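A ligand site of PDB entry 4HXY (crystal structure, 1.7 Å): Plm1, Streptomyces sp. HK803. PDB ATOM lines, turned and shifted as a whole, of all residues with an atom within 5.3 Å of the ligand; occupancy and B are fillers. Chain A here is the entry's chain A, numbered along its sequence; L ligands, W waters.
The backbone carbonyl oxygen (O) of Lys 300 lies within hydrogen-bond range of a ring nitrogen (NE2) of His 275, at 2.8 Å.
The side-chain carboxylate (OD1) of Asp 249 is in hydrogen-bond range of the side-chain hydroxyl (OG1) of Thr 251 (2.9 Å).
The side-chain hydroxyl of Ser 321 is in hydrogen-bond range of the backbone carbonyl oxygen of Asn 339, 3.2 Å away.
O of Ser 220 lies within hydrogen-bond range of N of Val 248 (2.9 Å).
OG of Ser 220 lies within hydrogen-bond range of N of Gly 223, 2.9 Å away.
The backbone NH of Gly 195 sits at hydrogen-bond distance from the backbone carbonyl oxygen of Leu 219, 3.2 Å away.
N of Ser 322 is in hydrogen-bond range of OD1 of Asn 339 (3.3 Å).
O of His 275 is in hydrogen-bond range of N of Phe 320 (3.1 Å).
N of Leu 199 sits at hydrogen-bond distance from O9 of the ligand, 2.7 Å away.
O17 of the ligand sits at hydrogen-bond distance from N of Arg 221, at 2.8 Å.
O17 of the ligand is in salt-bridge range of NE of Arg 221 (2.7 Å).
The side-chain hydroxyl (OH) of Tyr 335 lies within hydrogen-bond range of an oxygen (O13) of the ligand, 2.8 Å away.
An oxygen (O14) of the ligand lies within hydrogen-bond range of the backbone NH (N) of Trp 364.
The backbone NH (N) of Gln 222 sits at hydrogen-bond distance from an oxygen (O15) of the ligand (3.0 Å).
The side-chain amide nitrogen (NE2) of Gln 222 sits at hydrogen-bond distance from an oxygen (O15) of the ligand (2.8 Å).
N of Met 369 lies within hydrogen-bond range of O8 of the ligand (2.9 Å).
The side-chain amino group (NZ) of Lys 300 lies within hydrogen-bond range of an oxygen (O12) of the ligand (2.9 Å).
The backbone NH (N) of Val 250 sits at hydrogen-bond distance from a nitrogen (N4) of the ligand (3.0 Å).
A nitrogen (N3) of the ligand sits at hydrogen-bond distance from the side-chain carboxylate (OD1) of Asp 249 (3.0 Å).
N of Gly 198 is in hydrogen-bond range of O1 of the ligand (3.0 Å).
O of Ala 276 lies close to O12 of the ligand.
The backbone NH (N) of Gly 197 lies within hydrogen-bond range of an oxygen (O5) of the ligand, 3.2 Å away.
O4 of the ligand lies within hydrogen-bond range of N of Gly 278, at 3.4 Å.
Residues that only touch the ligand: Gly 194, Thr 196, Leu 219, Ser 220, Val 248, Ala 277, Ala 299, Phe 320, Ser 321, Ser 322, Trp 361, Gly 362, Pro 363, Gly 368 and Leu 370.
Hydrophobic or aromatic side chains within 4 Å of the ligand: Leu 199, Leu 219, Val 250, Ala 276, Ala 277, Ala 299, Tyr 335, Trp 361, Trp 364, Met 369 and Leu 370.
Water W3 bridges O2 of the ligand (2.6 Å) and O of Gly 278 (2.8 Å).
Water W9 lies within hydrogen-bond range of a nitrogen (N2) of the ligand and the guanidinium group of Arg 221.
Water W10 bridges OG1 of Thr 196 (2.6 Å) and O5 of the ligand (2.8 Å).
Water W4 lies within hydrogen-bond range of the backbone carbonyl oxygen (O) of Gly 367 (2.7 Å), a nitrogen (N7) of the ligand (2.9 Å) and the backbone NH (N) of Leu 370 (3.3 Å).
Water W7 lies within hydrogen-bond range of N of Gly 200, O of Gly 194, O9 of the ligand and N of Leu 199.
Water W5 bridges the side-chain hydroxyl (OH) of Tyr 335 (2.6 Å) and the side-chain hydroxyl (OG) of Ser 322 (2.7 Å).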
ATOM      1  N   GLY A 194     -25.600 -23.802  10.345  1.00  0.00           N
ATOM      2  CA  GLY A 194     -26.990 -23.586   9.979  1.00  0.00           C
ATOM      3  C   GLY A 194     -27.883 -23.401  11.207  1.00  0.00           C
ATOM      4  O   GLY A 194     -29.063 -23.692  11.152  1.00  0.00           O
ATOM      5  N   GLY A 195     -27.305 -22.910  12.302  1.00  0.00           N
ATOM      6  CA  GLY A 195     -27.964 -22.923  13.618  1.00  0.00           C
ATOM      7  C   GLY A 195     -29.147 -21.975  13.737  1.00  0.00           C
ATOM      8  O   GLY A 195     -29.994 -22.176  14.580  1.00  0.00           O
ATOM      9  N   THR A 196     -29.216 -20.965  12.872  1.00  0.00           N
ATOM     10  CA  THR A 196     -30.361 -20.036  12.860  1.00  0.00           C
ATOM     11  C   THR A 196     -31.426 -20.458  11.850  1.00  0.00           C
ATOM     12  O   THR A 196     -32.481 -19.822  11.753  1.00  0.00           O
ATOM     13  CB  THR A 196     -29.901 -18.618  12.512  1.00  0.00           C
ATOM     14  OG1 THR A 196     -29.095 -18.647  11.328  1.00  0.00           O
ATOM     15  CG2 THR A 196     -29.078 -17.998  13.678  1.00  0.00           C
ATOM     16  N   GLY A 197     -31.157 -21.536  11.115  1.00  0.00           N
ATOM     17  CA  GLY A 197     -32.135 -22.172  10.244  1.00  0.00           C
ATOM     18  C   GLY A 197     -33.178 -22.975  10.979  1.00  0.00           C
ATOM     19  O   GLY A 197     -33.210 -22.994  12.220  1.00  0.00           O
ATOM     20  N   GLY A 198     -34.036 -23.658  10.225  1.00  0.00           N
ATOM     21  CA  GLY A 198     -35.156 -24.375  10.791  1.00  0.00           C
ATOM     22  C   GLY A 198     -34.727 -25.506  11.689  1.00  0.00           C
ATOM     23  O   GLY A 198     -35.010 -25.517  12.886  1.00  0.00           O
ATOM     24  N   LEU A 199     -34.014 -26.473  11.105  1.00  0.00           N
ATOM     25  CA  LEU A 199     -33.620 -27.666  11.858  1.00  0.00           C
ATOM     26  C   LEU A 199     -32.574 -27.308  12.896  1.00  0.00           C
ATOM     27  O   LEU A 199     -32.640 -27.808  14.040  1.00  0.00           O
ATOM     28  CB  LEU A 199     -33.128 -28.779  10.951  1.00  0.00           C
ATOM     29  CG  LEU A 199     -34.216 -29.725  10.425  1.00  0.00           C
ATOM     30  CD1 LEU A 199     -35.400 -29.004   9.768  1.00  0.00           C
ATOM     31  CD2 LEU A 199     -33.604 -30.765   9.487  1.00  0.00           C
ATOM     32  N   GLY A 200     -31.616 -26.457  12.512  1.00  0.00           N
ATOM     33  CA  GLY A 200     -30.595 -25.950  13.449  1.00  0.00           C
ATOM     34  C   GLY A 200     -31.218 -25.375  14.708  1.00  0.00           C
ATOM     35  O   GLY A 200     -30.743 -25.617  15.828  1.00  0.00           O
ATOM     36  N   LEU A 219     -24.154 -20.961  14.073  1.00  0.00           N
ATOM     37  CA  LEU A 219     -23.318 -20.411  12.982  1.00  0.00           C
ATOM     38  C   LEU A 219     -24.069 -20.422  11.659  1.00  0.00           C
ATOM     39  O   LEU A 219     -24.652 -21.431  11.257  1.00  0.00           O
ATOM     40  CB  LEU A 219     -22.036 -21.253  12.855  1.00  0.00           C
ATOM     41  CG  LEU A 219     -20.987 -20.824  11.831  1.00  0.00           C
ATOM     42  CD1 LEU A 219     -19.594 -21.253  12.260  1.00  0.00           C
ATOM     43  CD2 LEU A 219     -21.320 -21.421  10.457  1.00  0.00           C
ATOM     44  N   SER A 220     -24.039 -19.278  10.973  1.00  0.00           N
ATOM     45  CA  SER A 220     -24.694 -19.135   9.659  1.00  0.00           C
ATOM     46  C   SER A 220     -24.104 -17.892   9.040  1.00  0.00           C
ATOM     47  O   SER A 220     -23.429 -17.132   9.724  1.00  0.00           O
ATOM     48  CB  SER A 220     -26.199 -19.047   9.785  1.00  0.00           C
ATOM     49  OG  SER A 220     -26.618 -17.845  10.414  1.00  0.00           O
ATOM     50  N   ARG A 221     -24.303 -17.681   7.740  1.00  0.00           N
ATOM     51  CA  ARG A 221     -23.759 -16.464   7.127  1.00  0.00           C
ATOM     52  C   ARG A 221     -24.428 -15.217   7.686  1.00  0.00           C
ATOM     53  O   ARG A 221     -23.783 -14.168   7.811  1.00  0.00           O
ATOM     54  CB  ARG A 221     -23.888 -16.501   5.624  1.00  0.00           C
ATOM     55  CG  ARG A 221     -23.018 -17.553   4.985  1.00  0.00           C
ATOM     56  CD  ARG A 221     -23.456 -17.919   3.577  1.00  0.00           C
ATOM     57  NE  ARG A 221     -24.839 -18.361   3.509  1.00  0.00           N
ATOM     58  CZ  ARG A 221     -25.436 -18.716   2.372  1.00  0.00           C
ATOM     59  NH1 ARG A 221     -24.758 -18.695   1.226  1.00  0.00           N
ATOM     60  NH2 ARG A 221     -26.706 -19.066   2.360  1.00  0.00           N
ATOM     61  N   GLN A 222     -25.692 -15.321   8.036  1.00  0.00           N
ATOM     62  CA  GLN A 222     -26.434 -14.174   8.566  1.00  0.00           C
ATOM     63  C   GLN A 222     -26.163 -13.942  10.039  1.00  0.00           C
ATOM     64  O   GLN A 222     -26.200 -12.803  10.506  1.00  0.00           O
ATOM     65  CB  GLN A 222     -27.921 -14.315   8.337  1.00  0.00           C
ATOM     66  CG  GLN A 222     -28.323 -14.102   6.888  1.00  0.00           C
ATOM     67  CD  GLN A 222     -29.745 -14.438   6.654  1.00  0.00           C
ATOM     68  OE1 GLN A 222     -30.620 -13.572   6.659  1.00  0.00           O
ATOM     69  NE2 GLN A 222     -30.018 -15.745   6.489  1.00  0.00           N
ATOM     70  N   GLY A 223     -25.924 -15.012  10.783  1.00  0.00           N
ATOM     71  CA  GLY A 223     -25.611 -14.869  12.207  1.00  0.00           C
ATOM     72  C   GLY A 223     -26.776 -14.229  12.934  1.00  0.00           C
ATOM     73  O   GLY A 223     -27.932 -14.590  12.736  1.00  0.00           O
ATOM     74  N   ALA A 226     -29.889 -13.028  11.052  1.00  0.00           N
ATOM     75  CA  ALA A 226     -30.904 -13.957  10.515  1.00  0.00           C
ATOM     76  C   ALA A 226     -32.324 -13.682  11.050  1.00  0.00           C
ATOM     77  O   ALA A 226     -32.505 -13.415  12.245  1.00  0.00           O
ATOM     78  CB  ALA A 226     -30.525 -15.414  10.808  1.00  0.00           C
ATOM     79  N   VAL A 248     -20.680 -16.397  10.095  1.00  0.00           N
ATOM     80  CA  VAL A 248     -19.506 -17.044   9.550  1.00  0.00           C
ATOM     81  C   VAL A 248     -19.924 -17.973   8.410  1.00  0.00           C
ATOM     82  O   VAL A 248     -20.909 -18.670   8.516  1.00  0.00           O
ATOM     83  CB  VAL A 248     -18.717 -17.869  10.630  1.00  0.00           C
ATOM     84  CG1 VAL A 248     -17.564 -18.651  10.027  1.00  0.00           C
ATOM     85  CG2 VAL A 248     -18.151 -16.954  11.730  1.00  0.00           C
ATOM     86  N   ASP A 249     -19.207 -17.883   7.297  1.00  0.00           N
ATOM     87  CA  ASP A 249     -19.325 -18.856   6.208  1.00  0.00           C
ATOM     88  C   ASP A 249     -18.573 -20.136   6.594  1.00  0.00           C
ATOM     89  O   ASP A 249     -17.364 -20.134   6.798  1.00  0.00           O
ATOM     90  CB  ASP A 249     -18.731 -18.218   4.957  1.00  0.00           C
ATOM     91  CG  ASP A 249     -18.892 -19.051   3.698  1.00  0.00           C
ATOM     92  OD1 ASP A 249     -19.196 -20.242   3.789  1.00  0.00           O
ATOM     93  OD2 ASP A 249     -18.689 -18.478   2.607  1.00  0.00           O
ATOM     94  N   VAL A 250     -19.304 -21.259   6.645  1.00  0.00           N
ATOM     95  CA  VAL A 250     -18.762 -22.542   7.104  1.00  0.00           C
ATOM     96  C   VAL A 250     -17.668 -23.084   6.168  1.00  0.00           C
ATOM     97  O   VAL A 250     -16.923 -23.986   6.558  1.00  0.00           O
ATOM     98  CB  VAL A 250     -19.893 -23.587   7.313  1.00  0.00           C
ATOM     99  CG1 VAL A 250     -20.465 -24.059   5.965  1.00  0.00           C
ATOM    100  CG2 VAL A 250     -19.418 -24.749   8.189  1.00  0.00           C
ATOM    101  N   THR A 251     -17.561 -22.524   4.963  1.00  0.00           N
ATOM    102  CA  THR A 251     -16.529 -22.911   4.014  1.00  0.00           C
ATOM    103  C   THR A 251     -15.285 -22.015   4.084  1.00  0.00           C
ATOM    104  O   THR A 251     -14.288 -22.288   3.414  1.00  0.00           O
ATOM    105  CB  THR A 251     -17.042 -22.882   2.534  1.00  0.00           C
ATOM    106  OG1 THR A 251     -17.247 -21.536   2.083  1.00  0.00           O
ATOM    107  CG2 THR A 251     -18.351 -23.679   2.372  1.00  0.00           C
ATOM    108  N   HIS A 275     -23.900 -30.347  12.111  1.00  0.00           N
ATOM    109  CA  HIS A 275     -23.720 -29.655  10.833  1.00  0.00           C
ATOM    110  C   HIS A 275     -25.028 -29.670  10.054  1.00  0.00           C
ATOM    111  O   HIS A 275     -25.351 -30.656   9.404  1.00  0.00           O
ATOM    112  CB  HIS A 275     -22.590 -30.318  10.045  1.00  0.00           C
ATOM    113  CG  HIS A 275     -22.298 -29.707   8.707  1.00  0.00           C
ATOM    114  ND1 HIS A 275     -22.048 -28.354   8.542  1.00  0.00           N
ATOM    115  CD2 HIS A 275     -22.118 -30.286   7.503  1.00  0.00           C
ATOM    116  CE1 HIS A 275     -21.780 -28.131   7.262  1.00  0.00           C
ATOM    117  NE2 HIS A 275     -21.776 -29.288   6.608  1.00  0.00           N
ATOM    118  N   ALA A 276     -25.760 -28.557  10.132  1.00  0.00           N
ATOM    119  CA  ALA A 276     -27.015 -28.395   9.412  1.00  0.00           C
ATOM    120  C   ALA A 276     -26.954 -27.313   8.324  1.00  0.00           C
ATOM    121  O   ALA A 276     -27.966 -27.044   7.671  1.00  0.00           O
ATOM    122  CB  ALA A 276     -28.135 -28.106  10.373  1.00  0.00           C
ATOM    123  N   ALA A 277     -25.787 -26.736   8.081  1.00  0.00           N
ATOM    124  CA  ALA A 277     -25.609 -25.796   6.961  1.00  0.00           C
ATOM    125  C   ALA A 277     -25.819 -26.499   5.631  1.00  0.00           C
ATOM    126  O   ALA A 277     -25.308 -27.595   5.399  1.00  0.00           O
ATOM    127  CB  ALA A 277     -24.228 -25.156   6.996  1.00  0.00           C
ATOM    128  N   GLY A 278     -26.527 -25.835   4.730  1.00  0.00           N
ATOM    129  CA  GLY A 278     -26.834 -26.404   3.434  1.00  0.00           C
ATOM    130  C   GLY A 278     -27.874 -25.585   2.701  1.00  0.00           C
ATOM    131  O   GLY A 278     -28.522 -24.706   3.274  1.00  0.00           O
ATOM    132  N   VAL A 279     -28.005 -25.887   1.416  1.00  0.00           N
ATOM    133  CA  VAL A 279     -29.005 -25.269   0.554  1.00  0.00           C
ATOM    134  C   VAL A 279     -29.637 -26.354  -0.281  1.00  0.00           C
ATOM    135  O   VAL A 279     -29.040 -27.425  -0.472  1.00  0.00           O
ATOM    136  CB  VAL A 279     -28.433 -24.183  -0.385  1.00  0.00           C
ATOM    137  CG1 VAL A 279     -27.769 -23.068   0.445  1.00  0.00           C
ATOM    138  CG2 VAL A 279     -27.465 -24.762  -1.381  1.00  0.00           C
ATOM    139  N   ALA A 299     -21.537 -25.491   1.045  1.00  0.00           N
ATOM    140  CA  ALA A 299     -21.759 -25.433   2.511  1.00  0.00           C
ATOM    141  C   ALA A 299     -21.806 -26.835   3.118  1.00  0.00           C
ATOM    142  O   ALA A 299     -21.212 -27.110   4.164  1.00  0.00           O
ATOM    143  CB  ALA A 299     -23.011 -24.650   2.866  1.00  0.00           C
ATOM    144  N   LYS A 300     -22.535 -27.733   2.458  1.00  0.00           N
ATOM    145  CA  LYS A 300     -22.749 -29.061   3.006  1.00  0.00           C
ATOM    146  C   LYS A 300     -21.439 -29.859   3.028  1.00  0.00           C
ATOM    147  O   LYS A 300     -20.978 -30.293   4.082  1.00  0.00           O
ATOM    148  CB  LYS A 300     -23.859 -29.764   2.220  1.00  0.00           C
ATOM    149  CG  LYS A 300     -24.295 -31.075   2.812  1.00  0.00           C
ATOM    150  CD  LYS A 300     -25.595 -31.592   2.156  1.00  0.00           C
ATOM    151  CE  LYS A 300     -26.889 -30.953   2.730  1.00  0.00           C
ATOM    152  NZ  LYS A 300     -27.201 -31.422   4.097  1.00  0.00           N
ATOM    153  N   PHE A 320     -26.293 -33.645   9.283  1.00  0.00           N
ATOM    154  CA  PHE A 320     -27.670 -33.729   8.837  1.00  0.00           C
ATOM    155  C   PHE A 320     -27.699 -33.971   7.329  1.00  0.00           C
ATOM    156  O   PHE A 320     -27.478 -33.055   6.518  1.00  0.00           O
ATOM    157  CB  PHE A 320     -28.430 -32.469   9.210  1.00  0.00           C
ATOM    158  CG  PHE A 320     -29.035 -32.510  10.582  1.00  0.00           C
ATOM    159  CD1 PHE A 320     -28.492 -33.253  11.614  1.00  0.00           C
ATOM    160  CD2 PHE A 320     -30.226 -31.835  10.820  1.00  0.00           C
ATOM    161  CE1 PHE A 320     -29.093 -33.309  12.871  1.00  0.00           C
ATOM    162  CE2 PHE A 320     -30.848 -31.884  12.073  1.00  0.00           C
ATOM    163  CZ  PHE A 320     -30.263 -32.610  13.100  1.00  0.00           C
ATOM    164  N   SER A 321     -27.928 -35.227   6.971  1.00  0.00           N
ATOM    165  CA  SER A 321     -28.046 -35.644   5.618  1.00  0.00           C
ATOM    166  C   SER A 321     -29.530 -35.778   5.226  1.00  0.00           C
ATOM    167  O   SER A 321     -30.398 -35.301   5.941  1.00  0.00           O
ATOM    168  CB  SER A 321     -27.251 -36.943   5.418  1.00  0.00           C
ATOM    169  OG  SER A 321     -27.220 -37.332   4.070  1.00  0.00           O
ATOM    170  N   SER A 322     -29.798 -36.430   4.101  1.00  0.00           N
ATOM    171  CA  SER A 322     -31.148 -36.484   3.535  1.00  0.00           C
ATOM    172  C   SER A 322     -31.356 -37.802   2.806  1.00  0.00           C
ATOM    173  O   SER A 322     -30.400 -38.349   2.248  1.00  0.00           O
ATOM    174  CB  SER A 322     -31.351 -35.365   2.519  1.00  0.00           C
ATOM    175  OG  SER A 322     -32.604 -35.501   1.860  1.00  0.00           O
ATOM    176  N   TYR A 335     -27.914 -31.643  -4.512  1.00  0.00           N
ATOM    177  CA  TYR A 335     -28.346 -31.880  -3.140  1.00  0.00           C
ATOM    178  C   TYR A 335     -28.048 -33.340  -2.783  1.00  0.00           C
ATOM    179  O   TYR A 335     -27.440 -33.654  -1.750  1.00  0.00           O
ATOM    180  CB  TYR A 335     -29.822 -31.587  -3.019  1.00  0.00           C
ATOM    181  CG  TYR A 335     -30.369 -31.630  -1.623  1.00  0.00           C
ATOM    182  CD1 TYR A 335     -29.850 -30.830  -0.628  1.00  0.00           C
ATOM    183  CD2 TYR A 335     -31.451 -32.446  -1.317  1.00  0.00           C
ATOM    184  CE1 TYR A 335     -30.370 -30.850   0.663  1.00  0.00           C
ATOM    185  CE2 TYR A 335     -31.976 -32.483  -0.059  1.00  0.00           C
ATOM    186  CZ  TYR A 335     -31.438 -31.669   0.930  1.00  0.00           C
ATOM    187  OH  TYR A 335     -31.982 -31.712   2.178  1.00  0.00           O
ATOM    188  N   ASN A 339     -25.289 -34.833   0.020  1.00  0.00           N
ATOM    189  CA  ASN A 339     -25.731 -35.669   1.122  1.00  0.00           C
ATOM    190  C   ASN A 339     -25.021 -37.028   1.119  1.00  0.00           C
ATOM    191  O   ASN A 339     -24.646 -37.530   2.173  1.00  0.00           O
ATOM    192  CB  ASN A 339     -27.249 -35.785   1.124  1.00  0.00           C
ATOM    193  CG  ASN A 339     -27.922 -34.524   1.637  1.00  0.00           C
ATOM    194  OD1 ASN A 339     -27.738 -34.159   2.791  1.00  0.00           O
ATOM    195  ND2 ASN A 339     -28.707 -33.854   0.797  1.00  0.00           N
ATOM    196  N   TRP A 361     -32.148 -37.813   6.893  1.00  0.00           N
ATOM    197  CA  TRP A 361     -33.510 -37.482   7.217  1.00  0.00           C
ATOM    198  C   TRP A 361     -34.469 -37.454   6.012  1.00  0.00           C
ATOM    199  O   TRP A 361     -34.169 -36.910   4.931  1.00  0.00           O
ATOM    200  CB  TRP A 361     -33.553 -36.089   7.812  1.00  0.00           C
ATOM    201  CG  TRP A 361     -32.770 -35.911   9.061  1.00  0.00           C
ATOM    202  CD1 TRP A 361     -31.625 -35.180   9.213  1.00  0.00           C
ATOM    203  CD2 TRP A 361     -33.137 -36.368  10.351  1.00  0.00           C
ATOM    204  NE1 TRP A 361     -31.235 -35.206  10.516  1.00  0.00           N
ATOM    205  CE2 TRP A 361     -32.148 -35.924  11.245  1.00  0.00           C
ATOM    206  CE3 TRP A 361     -34.181 -37.127  10.832  1.00  0.00           C
ATOM    207  CZ2 TRP A 361     -32.189 -36.215  12.605  1.00  0.00           C
ATOM    208  CZ3 TRP A 361     -34.235 -37.406  12.178  1.00  0.00           C
ATOM    209  CH2 TRP A 361     -33.236 -36.969  13.056  1.00  0.00           C
ATOM    210  N   GLY A 362     -35.670 -37.990   6.243  1.00  0.00           N
ATOM    211  CA  GLY A 362     -36.833 -37.556   5.480  1.00  0.00           C
ATOM    212  C   GLY A 362     -37.249 -36.143   5.839  1.00  0.00           C
ATOM    213  O   GLY A 362     -36.627 -35.475   6.666  1.00  0.00           O
ATOM    214  N   PRO A 363     -38.330 -35.663   5.219  1.00  0.00           N
ATOM    215  CA  PRO A 363     -38.786 -34.316   5.457  1.00  0.00           C
ATOM    216  C   PRO A 363     -39.187 -34.137   6.913  1.00  0.00           C
ATOM    217  O   PRO A 363     -39.680 -35.078   7.543  1.00  0.00           O
ATOM    218  CB  PRO A 363     -39.988 -34.172   4.529  1.00  0.00           C
ATOM    219  CG  PRO A 363     -40.429 -35.567   4.246  1.00  0.00           C
ATOM    220  CD  PRO A 363     -39.179 -36.372   4.247  1.00  0.00           C
ATOM    221  N   TRP A 364     -38.921 -32.946   7.433  1.00  0.00           N
ATOM    222  CA  TRP A 364     -39.410 -32.541   8.756  1.00  0.00           C
ATOM    223  C   TRP A 364     -40.560 -31.568   8.636  1.00  0.00           C
ATOM    224  O   TRP A 364     -40.601 -30.735   7.737  1.00  0.00           O
ATOM    225  CB  TRP A 364     -38.320 -31.757   9.485  1.00  0.00           C
ATOM    226  CG  TRP A 364     -37.158 -32.532  10.052  1.00  0.00           C
ATOM    227  CD1 TRP A 364     -36.401 -33.502   9.421  1.00  0.00           C
ATOM    228  CD2 TRP A 364     -36.554 -32.313  11.323  1.00  0.00           C
ATOM    229  NE1 TRP A 364     -35.381 -33.906  10.258  1.00  0.00           N
ATOM    230  CE2 TRP A 364     -35.441 -33.183  11.415  1.00  0.00           C
ATOM    231  CE3 TRP A 364     -36.839 -31.470  12.393  1.00  0.00           C
ATOM    232  CZ2 TRP A 364     -34.638 -33.249  12.552  1.00  0.00           C
ATOM    233  CZ3 TRP A 364     -36.014 -31.513  13.522  1.00  0.00           C
ATOM    234  CH2 TRP A 364     -34.934 -32.399  13.587  1.00  0.00           C
ATOM    235  N   GLY A 367     -41.063 -25.980   9.592  1.00  0.00           N
ATOM    236  CA  GLY A 367     -40.265 -24.894   9.003  1.00  0.00           C
ATOM    237  C   GLY A 367     -38.902 -25.325   8.509  1.00  0.00           C
ATOM    238  O   GLY A 367     -38.458 -26.443   8.778  1.00  0.00           O
ATOM    239  N   GLY A 368     -38.259 -24.423   7.775  1.00  0.00           N
ATOM    240  CA  GLY A 368     -36.954 -24.692   7.193  1.00  0.00           C
ATOM    241  C   GLY A 368     -37.062 -24.664   5.676  1.00  0.00           C
ATOM    242  O   GLY A 368     -37.652 -23.745   5.101  1.00  0.00           O
ATOM    243  N   MET A 369     -36.487 -25.685   5.030  1.00  0.00           N
ATOM    244  CA  MET A 369     -36.445 -25.758   3.572  1.00  0.00           C
ATOM    245  C   MET A 369     -37.799 -25.953   2.937  1.00  0.00           C
ATOM    246  O   MET A 369     -38.049 -25.473   1.819  1.00  0.00           O
ATOM    247  CB  MET A 369     -35.546 -26.916   3.130  1.00  0.00           C
ATOM    248  CG  MET A 369     -34.099 -26.609   3.266  1.00  0.00           C
ATOM    249  SD  MET A 369     -33.079 -28.038   2.898  1.00  0.00           S
ATOM    250  CE  MET A 369     -31.464 -27.235   2.848  1.00  0.00           C
ATOM    251  N   LEU A 370     -38.678 -26.667   3.636  1.00  0.00           N
ATOM    252  CA  LEU A 370     -39.954 -27.071   3.047  1.00  0.00           C
ATOM    253  C   LEU A 370     -41.024 -26.011   3.263  1.00  0.00           C
ATOM    254  O   LEU A 370     -41.206 -25.515   4.377  1.00  0.00           O
ATOM    255  CB  LEU A 370     -40.421 -28.403   3.642  1.00  0.00           C
ATOM    256  CG  LEU A 370     -39.435 -29.562   3.539  1.00  0.00           C
ATOM    257  CD1 LEU A 370     -40.029 -30.807   4.145  1.00  0.00           C
ATOM    258  CD2 LEU A 370     -39.010 -29.809   2.100  1.00  0.00           C
HETATM  259  P1  LIG L   1     -32.679 -23.912   6.368  1.00  0.00           P
HETATM  260  O1  LIG L   1     -33.730 -23.360   7.263  1.00  0.00           O
HETATM  261  O2  LIG L   1     -32.475 -23.285   5.021  1.00  0.00           O
HETATM  262  O3  LIG L   1     -31.278 -23.908   7.134  1.00  0.00           O
HETATM  263  C1  LIG L   1     -30.064 -23.961   6.421  1.00  0.00           C
HETATM  264  C2  LIG L   1     -29.039 -23.146   7.147  1.00  0.00           C
HETATM  265  O4  LIG L   1     -27.796 -23.216   6.495  1.00  0.00           O
HETATM  266  C3  LIG L   1     -29.386 -21.680   7.204  1.00  0.00           C
HETATM  267  O5  LIG L   1     -29.235 -21.239   8.568  1.00  0.00           O
HETATM  268  C4  LIG L   1     -28.366 -20.999   6.308  1.00  0.00           C
HETATM  269  O6  LIG L   1     -28.200 -19.704   6.859  1.00  0.00           O
HETATM  270  C5  LIG L   1     -27.189 -21.948   6.483  1.00  0.00           C
HETATM  271  N1  LIG L   1     -26.133 -21.869   5.482  1.00  0.00           N
HETATM  272  C6  LIG L   1     -26.230 -22.059   4.123  1.00  0.00           C
HETATM  273  N2  LIG L   1     -25.020 -21.873   3.570  1.00  0.00           N
HETATM  274  C7  LIG L   1     -24.123 -21.590   4.572  1.00  0.00           C
HETATM  275  C8  LIG L   1     -22.755 -21.335   4.595  1.00  0.00           C
HETATM  276  N3  LIG L   1     -21.978 -21.310   3.520  1.00  0.00           N
HETATM  277  N4  LIG L   1     -22.170 -21.077   5.814  1.00  0.00           N
HETATM  278  C9  LIG L   1     -22.915 -21.111   6.999  1.00  0.00           C
HETATM  279  N5  LIG L   1     -24.260 -21.351   6.984  1.00  0.00           N
HETATM  280  C10 LIG L   1     -24.838 -21.598   5.776  1.00  0.00           C
HETATM  281  O7  LIG L   1     -32.914 -25.480   6.097  1.00  0.00           O
HETATM  282  P2  LIG L   1     -33.370 -26.607   7.123  1.00  0.00           P
HETATM  283  O8  LIG L   1     -34.598 -27.212   6.571  1.00  0.00           O
HETATM  284  O9  LIG L   1     -33.361 -26.163   8.535  1.00  0.00           O
HETATM  285  O10 LIG L   1     -32.280 -27.751   6.891  1.00  0.00           O
HETATM  286  C11 LIG L   1     -31.039 -27.743   7.533  1.00  0.00           C
HETATM  287  C12 LIG L   1     -30.274 -28.991   7.121  1.00  0.00           C
HETATM  288  O11 LIG L   1     -31.096 -30.141   7.263  1.00  0.00           O
HETATM  289  C13 LIG L   1     -29.843 -28.951   5.680  1.00  0.00           C
HETATM  290  O12 LIG L   1     -28.502 -29.333   5.588  1.00  0.00           O
HETATM  291  C14 LIG L   1     -30.713 -29.962   4.980  1.00  0.00           C
HETATM  292  O13 LIG L   1     -30.095 -30.551   3.848  1.00  0.00           O
HETATM  293  C15 LIG L   1     -31.027 -30.935   6.091  1.00  0.00           C
HETATM  294  N6  LIG L   1     -32.326 -31.603   5.895  1.00  0.00           N
HETATM  295  C16 LIG L   1     -33.494 -30.922   6.045  1.00  0.00           C
HETATM  296  C17 LIG L   1     -34.731 -31.477   5.716  1.00  0.00           C
HETATM  297  C18 LIG L   1     -36.001 -30.766   5.953  1.00  0.00           C
HETATM  298  O14 LIG L   1     -37.153 -31.508   5.790  1.00  0.00           O
HETATM  299  N7  LIG L   1     -36.107 -29.485   6.270  1.00  0.00           N
HETATM  300  C19 LIG L   1     -34.789 -32.964   5.494  1.00  0.00           C
HETATM  301  C20 LIG L   1     -33.452 -33.623   5.352  1.00  0.00           C
HETATM  302  C21 LIG L   1     -32.284 -32.937   5.585  1.00  0.00           C
HETATM  303  P3  LIG L   1     -27.486 -18.502   6.083  1.00  0.00           P
HETATM  304  O15 LIG L   1     -27.704 -17.300   6.973  1.00  0.00           O
HETATM  305  O16 LIG L   1     -28.104 -18.302   4.694  1.00  0.00           O
HETATM  306  O17 LIG L   1     -26.059 -18.805   5.887  1.00  0.00           O
HETATM  307  O   HOH W   1     -27.206 -15.540   3.405  1.00  0.00           O
HETATM  308  O   HOH W   2     -34.939 -21.127   7.386  1.00  0.00           O
HETATM  309  O   HOH W   3     -30.960 -23.386   2.908  1.00  0.00           O
HETATM  310  O   HOH W   4     -38.577 -28.038   6.665  1.00  0.00           O
HETATM  311  O   HOH W   5     -34.101 -33.274   2.170  1.00  0.00           O
HETATM  312  O   HOH W   6     -30.695 -18.750   4.152  1.00  0.00           O
HETATM  313  O   HOH W   7     -30.878 -25.507  10.006  1.00  0.00           O
HETATM  314  O   HOH W   8     -25.451 -30.269   6.182  1.00  0.00           O
HETATM  315  O   HOH W   9     -24.559 -22.160   0.816  1.00  0.00           O
HETATM  316  O   HOH W  10     -30.059 -18.578   8.925  1.00  0.00           O
HETATM  317  O   HOH W  11     -34.698 -22.650   3.515  1.00  0.00           O
HETATM  318  O   HOH W  12     -21.664 -21.444   0.503  1.00  0.00           O
